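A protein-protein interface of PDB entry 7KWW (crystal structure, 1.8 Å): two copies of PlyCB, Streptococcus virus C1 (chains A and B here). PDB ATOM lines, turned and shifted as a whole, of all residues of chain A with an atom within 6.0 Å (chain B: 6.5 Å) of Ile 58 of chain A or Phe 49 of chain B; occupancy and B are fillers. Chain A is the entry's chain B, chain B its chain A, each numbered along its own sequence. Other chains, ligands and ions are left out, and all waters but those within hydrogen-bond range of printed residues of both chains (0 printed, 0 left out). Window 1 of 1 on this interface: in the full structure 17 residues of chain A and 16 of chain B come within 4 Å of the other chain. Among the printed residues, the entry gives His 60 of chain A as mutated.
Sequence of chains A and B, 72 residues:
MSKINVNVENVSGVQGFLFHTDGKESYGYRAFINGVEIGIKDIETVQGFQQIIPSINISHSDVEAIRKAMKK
The backbone NH (N) of Ile 38 of chain B sits at hydrogen-bond distance from the backbone carbonyl oxygen (O) of Ala 31 of chain B (2.9 Å).
OD2 of Asp 62 of chain A lies within hydrogen-bond range of OG of Ser 59 of chain A.
O of His 20 of chain A lies within hydrogen-bond range of N of Ile 58 of chain A, 2.9 Å away.
The backbone NH (N) of Ile 56 of chain A is in hydrogen-bond range of the backbone carbonyl oxygen (O) of Leu 18 of chain A, 2.9 Å away.
N of Thr 21 of chain A sits at hydrogen-bond distance from OH of Tyr 27 of chain A (3.5 Å).
A ring nitrogen (NE2) of His 20 of chain A is in hydrogen-bond range of the side-chain carboxylate of Asp 22 of chain A.
Position printed for both chains: 18.
Of the 15 pairs that touch across the chains among the printed residues, none has its exchanged pair printed and touching as well.
The side-chain hydroxyl of Thr 45 of chain B sits at hydrogen-bond distance from the backbone NH of Ser 59 of chain A (2.9 Å).
N of Asp 22 of chain A sits at hydrogen-bond distance from OE2 of Glu 44 of chain B (2.8 Å).
ND2 of Asn 57 of chain A sits at hydrogen-bond distance from OE2 of Glu 44 of chain B.
The side-chain hydroxyl (OG1) of Thr 45 of chain B lies within hydrogen-bond range of the side-chain carboxylate (OD2) of Asp 62 of chain A (2.6 Å).
The side-chain carboxylate (OE1) of Glu 44 of chain B sits at hydrogen-bond distance from the side-chain hydroxyl (OG1) of Thr 21 of chain A (2.6 Å).
Among the printed residues, merely in contact across the chains: Phe 17 of chain A with Val 14 of chain B (3.5 Å), Ile 56 of chain A with Gly 48 of chain B (3.4 Å), Asn 57 of chain A with Thr 45 of chain B (3.7 Å), Asn 57 of chain A with Gly 48 of chain B (3.4 Å), Ile 58 of chain A with Thr 45 of chain B (3.8 Å), Ile 58 of chain A with Phe 49 of chain B (3.9 Å), Ser 59 of chain A with Glu 44 of chain B (3.6 Å), Asp 62 of chain A with Ile 40 of chain B (3.6 Å), Ile 66 of chain A with Ile 38 of chain B (3.4 Å) and Ile 66 of chain A with Phe 49 of chain B (3.6 Å).
Of chain B, only Thr 45 and Phe 49 come within 4 Å of Ile 58 of chain A.
Of the printed residues of chain A, Ile 38 of chain B touches Ile 66.
Of the printed residues of chain B, Asp 22 of chain A touches Glu 44.
Of the printed residues of chain A, Val 14 of chain B touches Phe 17.
Gln 50 of chain B touches none of the printed residues of chain A.
The nearest residue of chain A that does not touch Phe 49 of chain B is Ile 56 of chain A (4.1 Å).
Of the 17 printed residues of chain B, 7 touch a printed residue of chain A.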
ATOM      1  N   PHE A  17      20.239 -15.673 -13.337  1.00  0.00           N
ATOM      2  CA  PHE A  17      20.952 -16.452 -12.353  1.00  0.00           C
ATOM      3  C   PHE A  17      22.162 -17.064 -13.015  1.00  0.00           C
ATOM      4  O   PHE A  17      22.157 -17.315 -14.229  1.00  0.00           O
ATOM      5  CB  PHE A  17      20.078 -17.573 -11.713  1.00  0.00           C
ATOM      6  CG  PHE A  17      19.465 -18.519 -12.690  1.00  0.00           C
ATOM      7  CD1 PHE A  17      20.145 -19.647 -13.106  1.00  0.00           C
ATOM      8  CD2 PHE A  17      18.167 -18.284 -13.164  1.00  0.00           C
ATOM      9  CE1 PHE A  17      19.543 -20.535 -14.008  1.00  0.00           C
ATOM     10  CE2 PHE A  17      17.552 -19.146 -14.047  1.00  0.00           C
ATOM     11  CZ  PHE A  17      18.233 -20.294 -14.483  1.00  0.00           C
ATOM     12  N   LEU A  18      23.165 -17.329 -12.185  1.00  0.00           N
ATOM     13  CA  LEU A  18      24.291 -18.175 -12.554  1.00  0.00           C
ATOM     14  C   LEU A  18      23.928 -19.633 -12.306  1.00  0.00           C
ATOM     15  O   LEU A  18      23.221 -19.954 -11.345  1.00  0.00           O
ATOM     16  CB  LEU A  18      25.500 -17.866 -11.692  1.00  0.00           C
ATOM     17  CG  LEU A  18      26.098 -16.471 -11.955  1.00  0.00           C
ATOM     18  CD1 LEU A  18      26.677 -15.918 -10.687  1.00  0.00           C
ATOM     19  CD2 LEU A  18      27.234 -16.715 -12.957  1.00  0.00           C
ATOM     20  N   PHE A  19      24.484 -20.520 -13.124  1.00  0.00           N
ATOM     21  CA  PHE A  19      24.275 -21.929 -12.856  1.00  0.00           C
ATOM     22  C   PHE A  19      25.517 -22.732 -13.177  1.00  0.00           C
ATOM     23  O   PHE A  19      26.269 -22.378 -14.083  1.00  0.00           O
ATOM     24  CB  PHE A  19      23.047 -22.469 -13.616  1.00  0.00           C
ATOM     25  CG  PHE A  19      23.060 -22.339 -15.147  1.00  0.00           C
ATOM     26  CD1 PHE A  19      22.681 -21.134 -15.760  1.00  0.00           C
ATOM     27  CD2 PHE A  19      23.277 -23.455 -15.954  1.00  0.00           C
ATOM     28  CE1 PHE A  19      22.622 -21.033 -17.159  1.00  0.00           C
ATOM     29  CE2 PHE A  19      23.207 -23.368 -17.365  1.00  0.00           C
ATOM     30  CZ  PHE A  19      22.862 -22.162 -17.958  1.00  0.00           C
ATOM     31  N   HIS A  20      25.729 -23.806 -12.409  1.00  0.00           N
ATOM     32  CA  HIS A  20      26.836 -24.738 -12.631  1.00  0.00           C
ATOM     33  C   HIS A  20      26.455 -26.082 -12.022  1.00  0.00           C
ATOM     34  O   HIS A  20      25.484 -26.180 -11.260  1.00  0.00           O
ATOM     35  CB  HIS A  20      28.150 -24.210 -12.020  1.00  0.00           C
ATOM     36  CG  HIS A  20      28.212 -24.318 -10.527  1.00  0.00           C
ATOM     37  ND1 HIS A  20      27.492 -23.470  -9.691  1.00  0.00           N
ATOM     38  CD2 HIS A  20      28.855 -25.190  -9.718  1.00  0.00           C
ATOM     39  CE1 HIS A  20      27.716 -23.812  -8.435  1.00  0.00           C
ATOM     40  NE2 HIS A  20      28.521 -24.866  -8.427  1.00  0.00           N
ATOM     41  N   THR A  21      27.227 -27.131 -12.348  1.00  0.00           N
ATOM     42  CA  THR A  21      27.072 -28.393 -11.623  1.00  0.00           C
ATOM     43  C   THR A  21      28.308 -28.733 -10.794  1.00  0.00           C
ATOM     44  O   THR A  21      29.451 -28.484 -11.200  1.00  0.00           O
ATOM     45  CB  THR A  21      26.742 -29.565 -12.562  1.00  0.00           C
ATOM     46  OG1 THR A  21      26.582 -30.763 -11.759  1.00  0.00           O
ATOM     47  CG2 THR A  21      27.846 -29.790 -13.583  1.00  0.00           C
ATOM     48  N   ASP A  22      28.077 -29.285  -9.613  1.00  0.00           N
ATOM     49  CA  ASP A  22      29.181 -29.877  -8.880  1.00  0.00           C
ATOM     50  C   ASP A  22      29.321 -31.372  -9.183  1.00  0.00           C
ATOM     51  O   ASP A  22      30.124 -32.036  -8.528  1.00  0.00           O
ATOM     52  CB  ASP A  22      29.000 -29.649  -7.383  1.00  0.00           C
ATOM     53  CG  ASP A  22      29.124 -28.206  -6.992  1.00  0.00           C
ATOM     54  OD1 ASP A  22      29.871 -27.460  -7.643  1.00  0.00           O
ATOM     55  OD2 ASP A  22      28.458 -27.813  -6.028  1.00  0.00           O
ATOM     56  N   TYR A  27      30.330 -28.237 -16.694  1.00  0.00           N
ATOM     57  CA  TYR A  27      30.276 -27.337 -17.826  1.00  0.00           C
ATOM     58  C   TYR A  27      30.730 -25.924 -17.428  1.00  0.00           C
ATOM     59  O   TYR A  27      30.449 -24.961 -18.143  1.00  0.00           O
ATOM     60  CB  TYR A  27      28.874 -27.276 -18.423  1.00  0.00           C
ATOM     61  CG  TYR A  27      27.781 -27.003 -17.426  1.00  0.00           C
ATOM     62  CD1 TYR A  27      27.498 -25.705 -17.036  1.00  0.00           C
ATOM     63  CD2 TYR A  27      27.062 -28.060 -16.845  1.00  0.00           C
ATOM     64  CE1 TYR A  27      26.483 -25.418 -16.069  1.00  0.00           C
ATOM     65  CE2 TYR A  27      26.033 -27.822 -15.910  1.00  0.00           C
ATOM     66  CZ  TYR A  27      25.763 -26.485 -15.531  1.00  0.00           C
ATOM     67  OH  TYR A  27      24.806 -26.194 -14.638  1.00  0.00           O
ATOM     68  N   ILE A  56      22.859 -20.804  -8.585  1.00  0.00           N
ATOM     69  CA  ILE A  56      22.271 -22.088  -8.185  1.00  0.00           C
ATOM     70  C   ILE A  56      22.953 -23.233  -8.917  1.00  0.00           C
ATOM     71  O   ILE A  56      23.732 -23.033  -9.852  1.00  0.00           O
ATOM     72  CB  ILE A  56      20.767 -22.144  -8.421  1.00  0.00           C
ATOM     73  CG1 ILE A  56      20.457 -22.061  -9.928  1.00  0.00           C
ATOM     74  CG2 ILE A  56      20.045 -21.045  -7.567  1.00  0.00           C
ATOM     75  CD1 ILE A  56      18.928 -22.304 -10.276  1.00  0.00           C
ATOM     76  N   ASN A  57      22.628 -24.464  -8.470  1.00  0.00           N
ATOM     77  CA  ASN A  57      23.179 -25.680  -9.057  1.00  0.00           C
ATOM     78  C   ASN A  57      22.164 -26.287 -10.006  1.00  0.00           C
ATOM     79  O   ASN A  57      20.993 -26.423  -9.644  1.00  0.00           O
ATOM     80  CB  ASN A  57      23.529 -26.721  -7.985  1.00  0.00           C
ATOM     81  CG  ASN A  57      24.742 -26.367  -7.256  1.00  0.00           C
ATOM     82  OD1 ASN A  57      24.806 -25.280  -6.652  1.00  0.00           O
ATOM     83  ND2 ASN A  57      25.753 -27.224  -7.328  1.00  0.00           N
ATOM     84  N   ILE A  58      22.621 -26.669 -11.196  1.00  0.00           N
ATOM     85  CA  ILE A  58      21.806 -27.360 -12.190  1.00  0.00           C
ATOM     86  C   ILE A  58      22.654 -28.464 -12.791  1.00  0.00           C
ATOM     87  O   ILE A  58      23.767 -28.209 -13.273  1.00  0.00           O
ATOM     88  CB  ILE A  58      21.323 -26.405 -13.300  1.00  0.00           C
ATOM     89  CG1 ILE A  58      20.469 -25.273 -12.716  1.00  0.00           C
ATOM     90  CG2 ILE A  58      20.573 -27.177 -14.407  1.00  0.00           C
ATOM     91  CD1 ILE A  58      20.015 -24.251 -13.735  1.00  0.00           C
ATOM     92  N   SER A  59      22.140 -29.688 -12.785  1.00  0.00           N
ATOM     93  CA  SER A  59      22.963 -30.762 -13.308  1.00  0.00           C
ATOM     94  C   SER A  59      23.060 -30.638 -14.817  1.00  0.00           C
ATOM     95  O   SER A  59      22.190 -30.050 -15.468  1.00  0.00           O
ATOM     96  CB  SER A  59      22.374 -32.125 -12.948  1.00  0.00           C
ATOM     97  OG  SER A  59      21.195 -32.282 -13.697  1.00  0.00           O
ATOM     98  N   HIS A  60      24.122 -31.228 -15.376  1.00  0.00           N
ATOM     99  CA  HIS A  60      24.315 -31.148 -16.813  1.00  0.00           C
ATOM    100  C   HIS A  60      23.104 -31.701 -17.552  1.00  0.00           C
ATOM    101  O   HIS A  60      22.657 -31.116 -18.550  1.00  0.00           O
ATOM    102  CB  HIS A  60      25.607 -31.874 -17.223  1.00  0.00           C
ATOM    103  CG  HIS A  60      26.055 -31.547 -18.618  1.00  0.00           C
ATOM    104  ND1 HIS A  60      25.179 -31.150 -19.607  1.00  0.00           N
ATOM    105  CD2 HIS A  60      27.290 -31.478 -19.171  1.00  0.00           C
ATOM    106  CE1 HIS A  60      25.846 -30.896 -20.719  1.00  0.00           C
ATOM    107  NE2 HIS A  60      27.130 -31.088 -20.482  1.00  0.00           N
ATOM    108  N   ASP A  62      20.040 -31.593 -16.823  1.00  0.00           N
ATOM    109  CA  ASP A  62      18.853 -30.746 -16.775  1.00  0.00           C
ATOM    110  C   ASP A  62      18.985 -29.430 -17.539  1.00  0.00           C
ATOM    111  O   ASP A  62      17.992 -28.707 -17.680  1.00  0.00           O
ATOM    112  CB  ASP A  62      18.497 -30.437 -15.312  1.00  0.00           C
ATOM    113  CG  ASP A  62      17.803 -31.641 -14.628  1.00  0.00           C
ATOM    114  OD1 ASP A  62      16.945 -32.271 -15.286  1.00  0.00           O
ATOM    115  OD2 ASP A  62      18.124 -31.968 -13.458  1.00  0.00           O
ATOM    116  N   VAL A  63      20.178 -29.079 -18.009  1.00  0.00           N
ATOM    117  CA  VAL A  63      20.339 -27.758 -18.621  1.00  0.00           C
ATOM    118  C   VAL A  63      19.449 -27.592 -19.853  1.00  0.00           C
ATOM    119  O   VAL A  63      18.884 -26.516 -20.085  1.00  0.00           O
ATOM    120  CB  VAL A  63      21.820 -27.533 -18.961  1.00  0.00           C
ATOM    121  CG1 VAL A  63      21.951 -26.334 -19.894  1.00  0.00           C
ATOM    122  CG2 VAL A  63      22.591 -27.303 -17.672  1.00  0.00           C
ATOM    123  N   ILE A  66      15.938 -26.580 -18.816  1.00  0.00           N
ATOM    124  CA  ILE A  66      15.919 -25.214 -18.294  1.00  0.00           C
ATOM    125  C   ILE A  66      16.052 -24.185 -19.428  1.00  0.00           C
ATOM    126  O   ILE A  66      15.436 -23.114 -19.398  1.00  0.00           O
ATOM    127  CB  ILE A  66      17.029 -25.010 -17.247  1.00  0.00           C
ATOM    128  CG1 ILE A  66      16.911 -26.006 -16.096  1.00  0.00           C
ATOM    129  CG2 ILE A  66      17.020 -23.543 -16.699  1.00  0.00           C
ATOM    130  CD1 ILE A  66      15.556 -26.154 -15.625  1.00  0.00           C
ATOM    131  N   VAL B  14      12.879 -15.785 -12.711  1.00  0.00           N
ATOM    132  CA  VAL B  14      12.147 -17.063 -12.762  1.00  0.00           C
ATOM    133  C   VAL B  14      10.903 -16.892 -11.918  1.00  0.00           C
ATOM    134  O   VAL B  14      11.023 -16.487 -10.763  1.00  0.00           O
ATOM    135  CB  VAL B  14      12.980 -18.211 -12.198  1.00  0.00           C
ATOM    136  CG1 VAL B  14      12.163 -19.542 -12.208  1.00  0.00           C
ATOM    137  CG2 VAL B  14      14.259 -18.405 -13.007  1.00  0.00           C
ATOM    138  N   LEU B  18       8.392 -25.869  -8.198  1.00  0.00           N
ATOM    139  CA  LEU B  18       8.602 -27.310  -8.313  1.00  0.00           C
ATOM    140  C   LEU B  18       7.367 -28.022  -7.802  1.00  0.00           C
ATOM    141  O   LEU B  18       6.702 -27.517  -6.884  1.00  0.00           O
ATOM    142  CB  LEU B  18       9.757 -27.735  -7.422  1.00  0.00           C
ATOM    143  CG  LEU B  18      11.074 -27.229  -7.987  1.00  0.00           C
ATOM    144  CD1 LEU B  18      12.016 -27.025  -6.820  1.00  0.00           C
ATOM    145  CD2 LEU B  18      11.636 -28.386  -8.753  1.00  0.00           C
ATOM    146  N   ALA B  31       8.616 -29.046 -12.775  1.00  0.00           N
ATOM    147  CA  ALA B  31       8.463 -27.638 -12.408  1.00  0.00           C
ATOM    148  C   ALA B  31       7.713 -26.907 -13.496  1.00  0.00           C
ATOM    149  O   ALA B  31       7.783 -27.305 -14.661  1.00  0.00           O
ATOM    150  CB  ALA B  31       9.856 -26.974 -12.233  1.00  0.00           C
ATOM    151  N   ILE B  33       8.281 -23.279 -15.009  1.00  0.00           N
ATOM    152  CA  ILE B  33       9.280 -22.212 -14.964  1.00  0.00           C
ATOM    153  C   ILE B  33       8.875 -21.241 -16.067  1.00  0.00           C
ATOM    154  O   ILE B  33       8.814 -21.631 -17.235  1.00  0.00           O
ATOM    155  CB  ILE B  33      10.685 -22.769 -15.144  1.00  0.00           C
ATOM    156  CG1 ILE B  33      11.094 -23.361 -13.766  1.00  0.00           C
ATOM    157  CG2 ILE B  33      11.701 -21.624 -15.404  1.00  0.00           C
ATOM    158  CD1 ILE B  33      12.306 -24.026 -13.743  1.00  0.00           C
ATOM    159  N   ILE B  38       8.534 -28.525 -17.160  1.00  0.00           N
ATOM    160  CA  ILE B  38       9.645 -29.431 -17.440  1.00  0.00           C
ATOM    161  C   ILE B  38       9.731 -30.537 -16.389  1.00  0.00           C
ATOM    162  O   ILE B  38       9.308 -30.391 -15.236  1.00  0.00           O
ATOM    163  CB  ILE B  38      10.966 -28.672 -17.458  1.00  0.00           C
ATOM    164  CG1 ILE B  38      11.183 -28.093 -16.090  1.00  0.00           C
ATOM    165  CG2 ILE B  38      10.941 -27.545 -18.465  1.00  0.00           C
ATOM    166  CD1 ILE B  38      12.411 -27.237 -16.059  1.00  0.00           C
ATOM    167  N   ILE B  40      12.417 -32.752 -14.130  1.00  0.00           N
ATOM    168  CA  ILE B  40      13.724 -32.479 -13.536  1.00  0.00           C
ATOM    169  C   ILE B  40      14.376 -33.816 -13.278  1.00  0.00           C
ATOM    170  O   ILE B  40      13.830 -34.634 -12.538  1.00  0.00           O
ATOM    171  CB  ILE B  40      13.589 -31.654 -12.258  1.00  0.00           C
ATOM    172  CG1 ILE B  40      13.100 -30.240 -12.632  1.00  0.00           C
ATOM    173  CG2 ILE B  40      14.943 -31.575 -11.540  1.00  0.00           C
ATOM    174  CD1 ILE B  40      12.985 -29.407 -11.519  1.00  0.00           C
ATOM    175  N   GLU B  44      20.381 -32.657  -7.664  1.00  0.00           N
ATOM    176  CA  GLU B  44      21.097 -31.378  -7.590  1.00  0.00           C
ATOM    177  C   GLU B  44      20.280 -30.219  -8.158  1.00  0.00           C
ATOM    178  O   GLU B  44      20.254 -29.117  -7.593  1.00  0.00           O
ATOM    179  CB  GLU B  44      22.413 -31.507  -8.330  1.00  0.00           C
ATOM    180  CG  GLU B  44      23.168 -30.188  -8.377  1.00  0.00           C
ATOM    181  CD  GLU B  44      24.478 -30.284  -9.177  1.00  0.00           C
ATOM    182  OE1 GLU B  44      24.561 -31.084 -10.128  1.00  0.00           O
ATOM    183  OE2 GLU B  44      25.426 -29.547  -8.848  1.00  0.00           O
ATOM    184  N   THR B  45      19.593 -30.442  -9.275  1.00  0.00           N
ATOM    185  CA  THR B  45      18.759 -29.405  -9.852  1.00  0.00           C
ATOM    186  C   THR B  45      17.573 -29.065  -8.947  1.00  0.00           C
ATOM    187  O   THR B  45      17.174 -27.910  -8.850  1.00  0.00           O
ATOM    188  CB  THR B  45      18.262 -29.863 -11.213  1.00  0.00           C
ATOM    189  OG1 THR B  45      19.402 -30.334 -11.945  1.00  0.00           O
ATOM    190  CG2 THR B  45      17.560 -28.739 -11.924  1.00  0.00           C
ATOM    191  N   VAL B  46      16.938 -30.081  -8.348  1.00  0.00           N
ATOM    192  CA  VAL B  46      15.845 -29.773  -7.419  1.00  0.00           C
ATOM    193  C   VAL B  46      16.346 -28.836  -6.326  1.00  0.00           C
ATOM    194  O   VAL B  46      15.719 -27.806  -6.035  1.00  0.00           O
ATOM    195  CB  VAL B  46      15.260 -31.075  -6.831  1.00  0.00           C
ATOM    196  CG1 VAL B  46      14.301 -30.737  -5.737  1.00  0.00           C
ATOM    197  CG2 VAL B  46      14.584 -31.959  -7.952  1.00  0.00           C
ATOM    198  N   GLN B  47      17.455 -29.192  -5.692  1.00  0.00           N
ATOM    199  CA  GLN B  47      17.985 -28.380  -4.608  1.00  0.00           C
ATOM    200  C   GLN B  47      18.409 -27.006  -5.099  1.00  0.00           C
ATOM    201  O   GLN B  47      18.215 -25.998  -4.387  1.00  0.00           O
ATOM    202  CB  GLN B  47      19.156 -29.116  -3.945  1.00  0.00           C
ATOM    203  CG  GLN B  47      18.688 -30.419  -3.437  1.00  0.00           C
ATOM    204  CD  GLN B  47      19.754 -31.213  -2.711  1.00  0.00           C
ATOM    205  OE1 GLN B  47      20.887 -31.308  -3.144  1.00  0.00           O
ATOM    206  NE2 GLN B  47      19.374 -31.771  -1.598  1.00  0.00           N
ATOM    207  N   GLY B  48      18.963 -26.928  -6.321  1.00  0.00           N
ATOM    208  CA  GLY B  48      19.247 -25.612  -6.897  1.00  0.00           C
ATOM    209  C   GLY B  48      17.996 -24.750  -7.002  1.00  0.00           C
ATOM    210  O   GLY B  48      17.959 -23.595  -6.551  1.00  0.00           O
ATOM    211  N   PHE B  49      16.966 -25.272  -7.653  1.00  0.00           N
ATOM    212  CA  PHE B  49      15.793 -24.425  -7.832  1.00  0.00           C
ATOM    213  C   PHE B  49      15.074 -24.159  -6.517  1.00  0.00           C
ATOM    214  O   PHE B  49      14.374 -23.139  -6.401  1.00  0.00           O
ATOM    215  CB  PHE B  49      14.880 -25.058  -8.884  1.00  0.00           C
ATOM    216  CG  PHE B  49      15.263 -24.632 -10.281  1.00  0.00           C
ATOM    217  CD1 PHE B  49      14.850 -23.402 -10.778  1.00  0.00           C
ATOM    218  CD2 PHE B  49      16.104 -25.401 -11.049  1.00  0.00           C
ATOM    219  CE1 PHE B  49      15.236 -22.981 -12.039  1.00  0.00           C
ATOM    220  CE2 PHE B  49      16.496 -24.986 -12.317  1.00  0.00           C
ATOM    221  CZ  PHE B  49      16.049 -23.782 -12.812  1.00  0.00           C
ATOM    222  N   GLN B  50      15.160 -25.077  -5.539  1.00  0.00           N
ATOM    223  CA  GLN B  50      14.527 -24.740  -4.268  1.00  0.00           C
ATOM    224  C   GLN B  50      15.144 -23.504  -3.647  1.00  0.00           C
ATOM    225  O   GLN B  50      14.565 -22.976  -2.696  1.00  0.00           O
ATOM    226  CB  GLN B  50      14.621 -25.902  -3.276  1.00  0.00           C
ATOM    227  CG  GLN B  50      13.584 -26.991  -3.650  1.00  0.00           C
ATOM    228  CD  GLN B  50      13.705 -28.262  -2.866  1.00  0.00           C
ATOM    229  OE1 GLN B  50      14.753 -28.568  -2.319  1.00  0.00           O
ATOM    230  NE2 GLN B  50      12.604 -29.065  -2.858  1.00  0.00           N
ATOM    231  N   GLN B  51      16.303 -23.036  -4.144  1.00  0.00           N
ATOM    232  CA  GLN B  51      16.825 -21.769  -3.624  1.00  0.00           C
ATOM    233  C   GLN B  51      16.060 -20.556  -4.120  1.00  0.00           C
ATOM    234  O   GLN B  51      16.089 -19.521  -3.442  1.00  0.00           O
ATOM    235  CB  GLN B  51      18.307 -21.586  -3.984  1.00  0.00           C
ATOM    236  CG  GLN B  51      19.188 -22.686  -3.436  1.00  0.00           C
ATOM    237  CD  GLN B  51      19.390 -22.540  -1.927  1.00  0.00           C
ATOM    238  OE1 GLN B  51      18.868 -23.324  -1.136  1.00  0.00           O
ATOM    239  NE2 GLN B  51      20.147 -21.522  -1.528  1.00  0.00           N
ATOM    240  N   ILE B  52      15.378 -20.643  -5.262  1.00  0.00           N
ATOM    241  CA  ILE B  52      14.739 -19.468  -5.847  1.00  0.00           C
ATOM    242  C   ILE B  52      13.231 -19.593  -6.082  1.00  0.00           C
ATOM    243  O   ILE B  52      12.584 -18.531  -6.286  1.00  0.00           O
ATOM    244  CB  ILE B  52      15.434 -19.070  -7.157  1.00  0.00           C
ATOM    245  CG1 ILE B  52      15.503 -20.239  -8.136  1.00  0.00           C
ATOM    246  CG2 ILE B  52      16.880 -18.645  -6.799  1.00  0.00           C
ATOM    247  CD1 ILE B  52      15.764 -19.775  -9.646  1.00  0.00           C
ATOM    248  N   ILE B  53      12.655 -20.787  -6.091  1.00  0.00           N
ATOM    249  CA  ILE B  53      11.197 -20.912  -6.295  1.00  0.00           C
ATOM    250  C   ILE B  53      10.616 -21.880  -5.283  1.00  0.00           C
ATOM    251  O   ILE B  53      11.309 -22.749  -4.725  1.00  0.00           O
ATOM    252  CB  ILE B  53      10.843 -21.366  -7.731  1.00  0.00           C
ATOM    253  CG1 ILE B  53      11.542 -22.679  -8.165  1.00  0.00           C
ATOM    254  CG2 ILE B  53      11.001 -20.201  -8.709  1.00  0.00           C
ATOM    255  CD1 ILE B  53      11.012 -23.210  -9.539  1.00  0.00           C
ATOM    256  N   PRO B  54       9.322 -21.745  -4.989  1.00  0.00           N
ATOM    257  CA  PRO B  54       8.706 -22.608  -3.991  1.00  0.00           C
ATOM    258  C   PRO B  54       8.586 -24.043  -4.505  1.00  0.00           C
ATOM    259  O   PRO B  54       8.619 -24.335  -5.708  1.00  0.00           O
ATOM    260  CB  PRO B  54       7.304 -22.000  -3.765  1.00  0.00           C
ATOM    261  CG  PRO B  54       7.090 -21.047  -4.874  1.00  0.00           C
ATOM    262  CD  PRO B  54       8.437 -20.652  -5.457  1.00  0.00           C
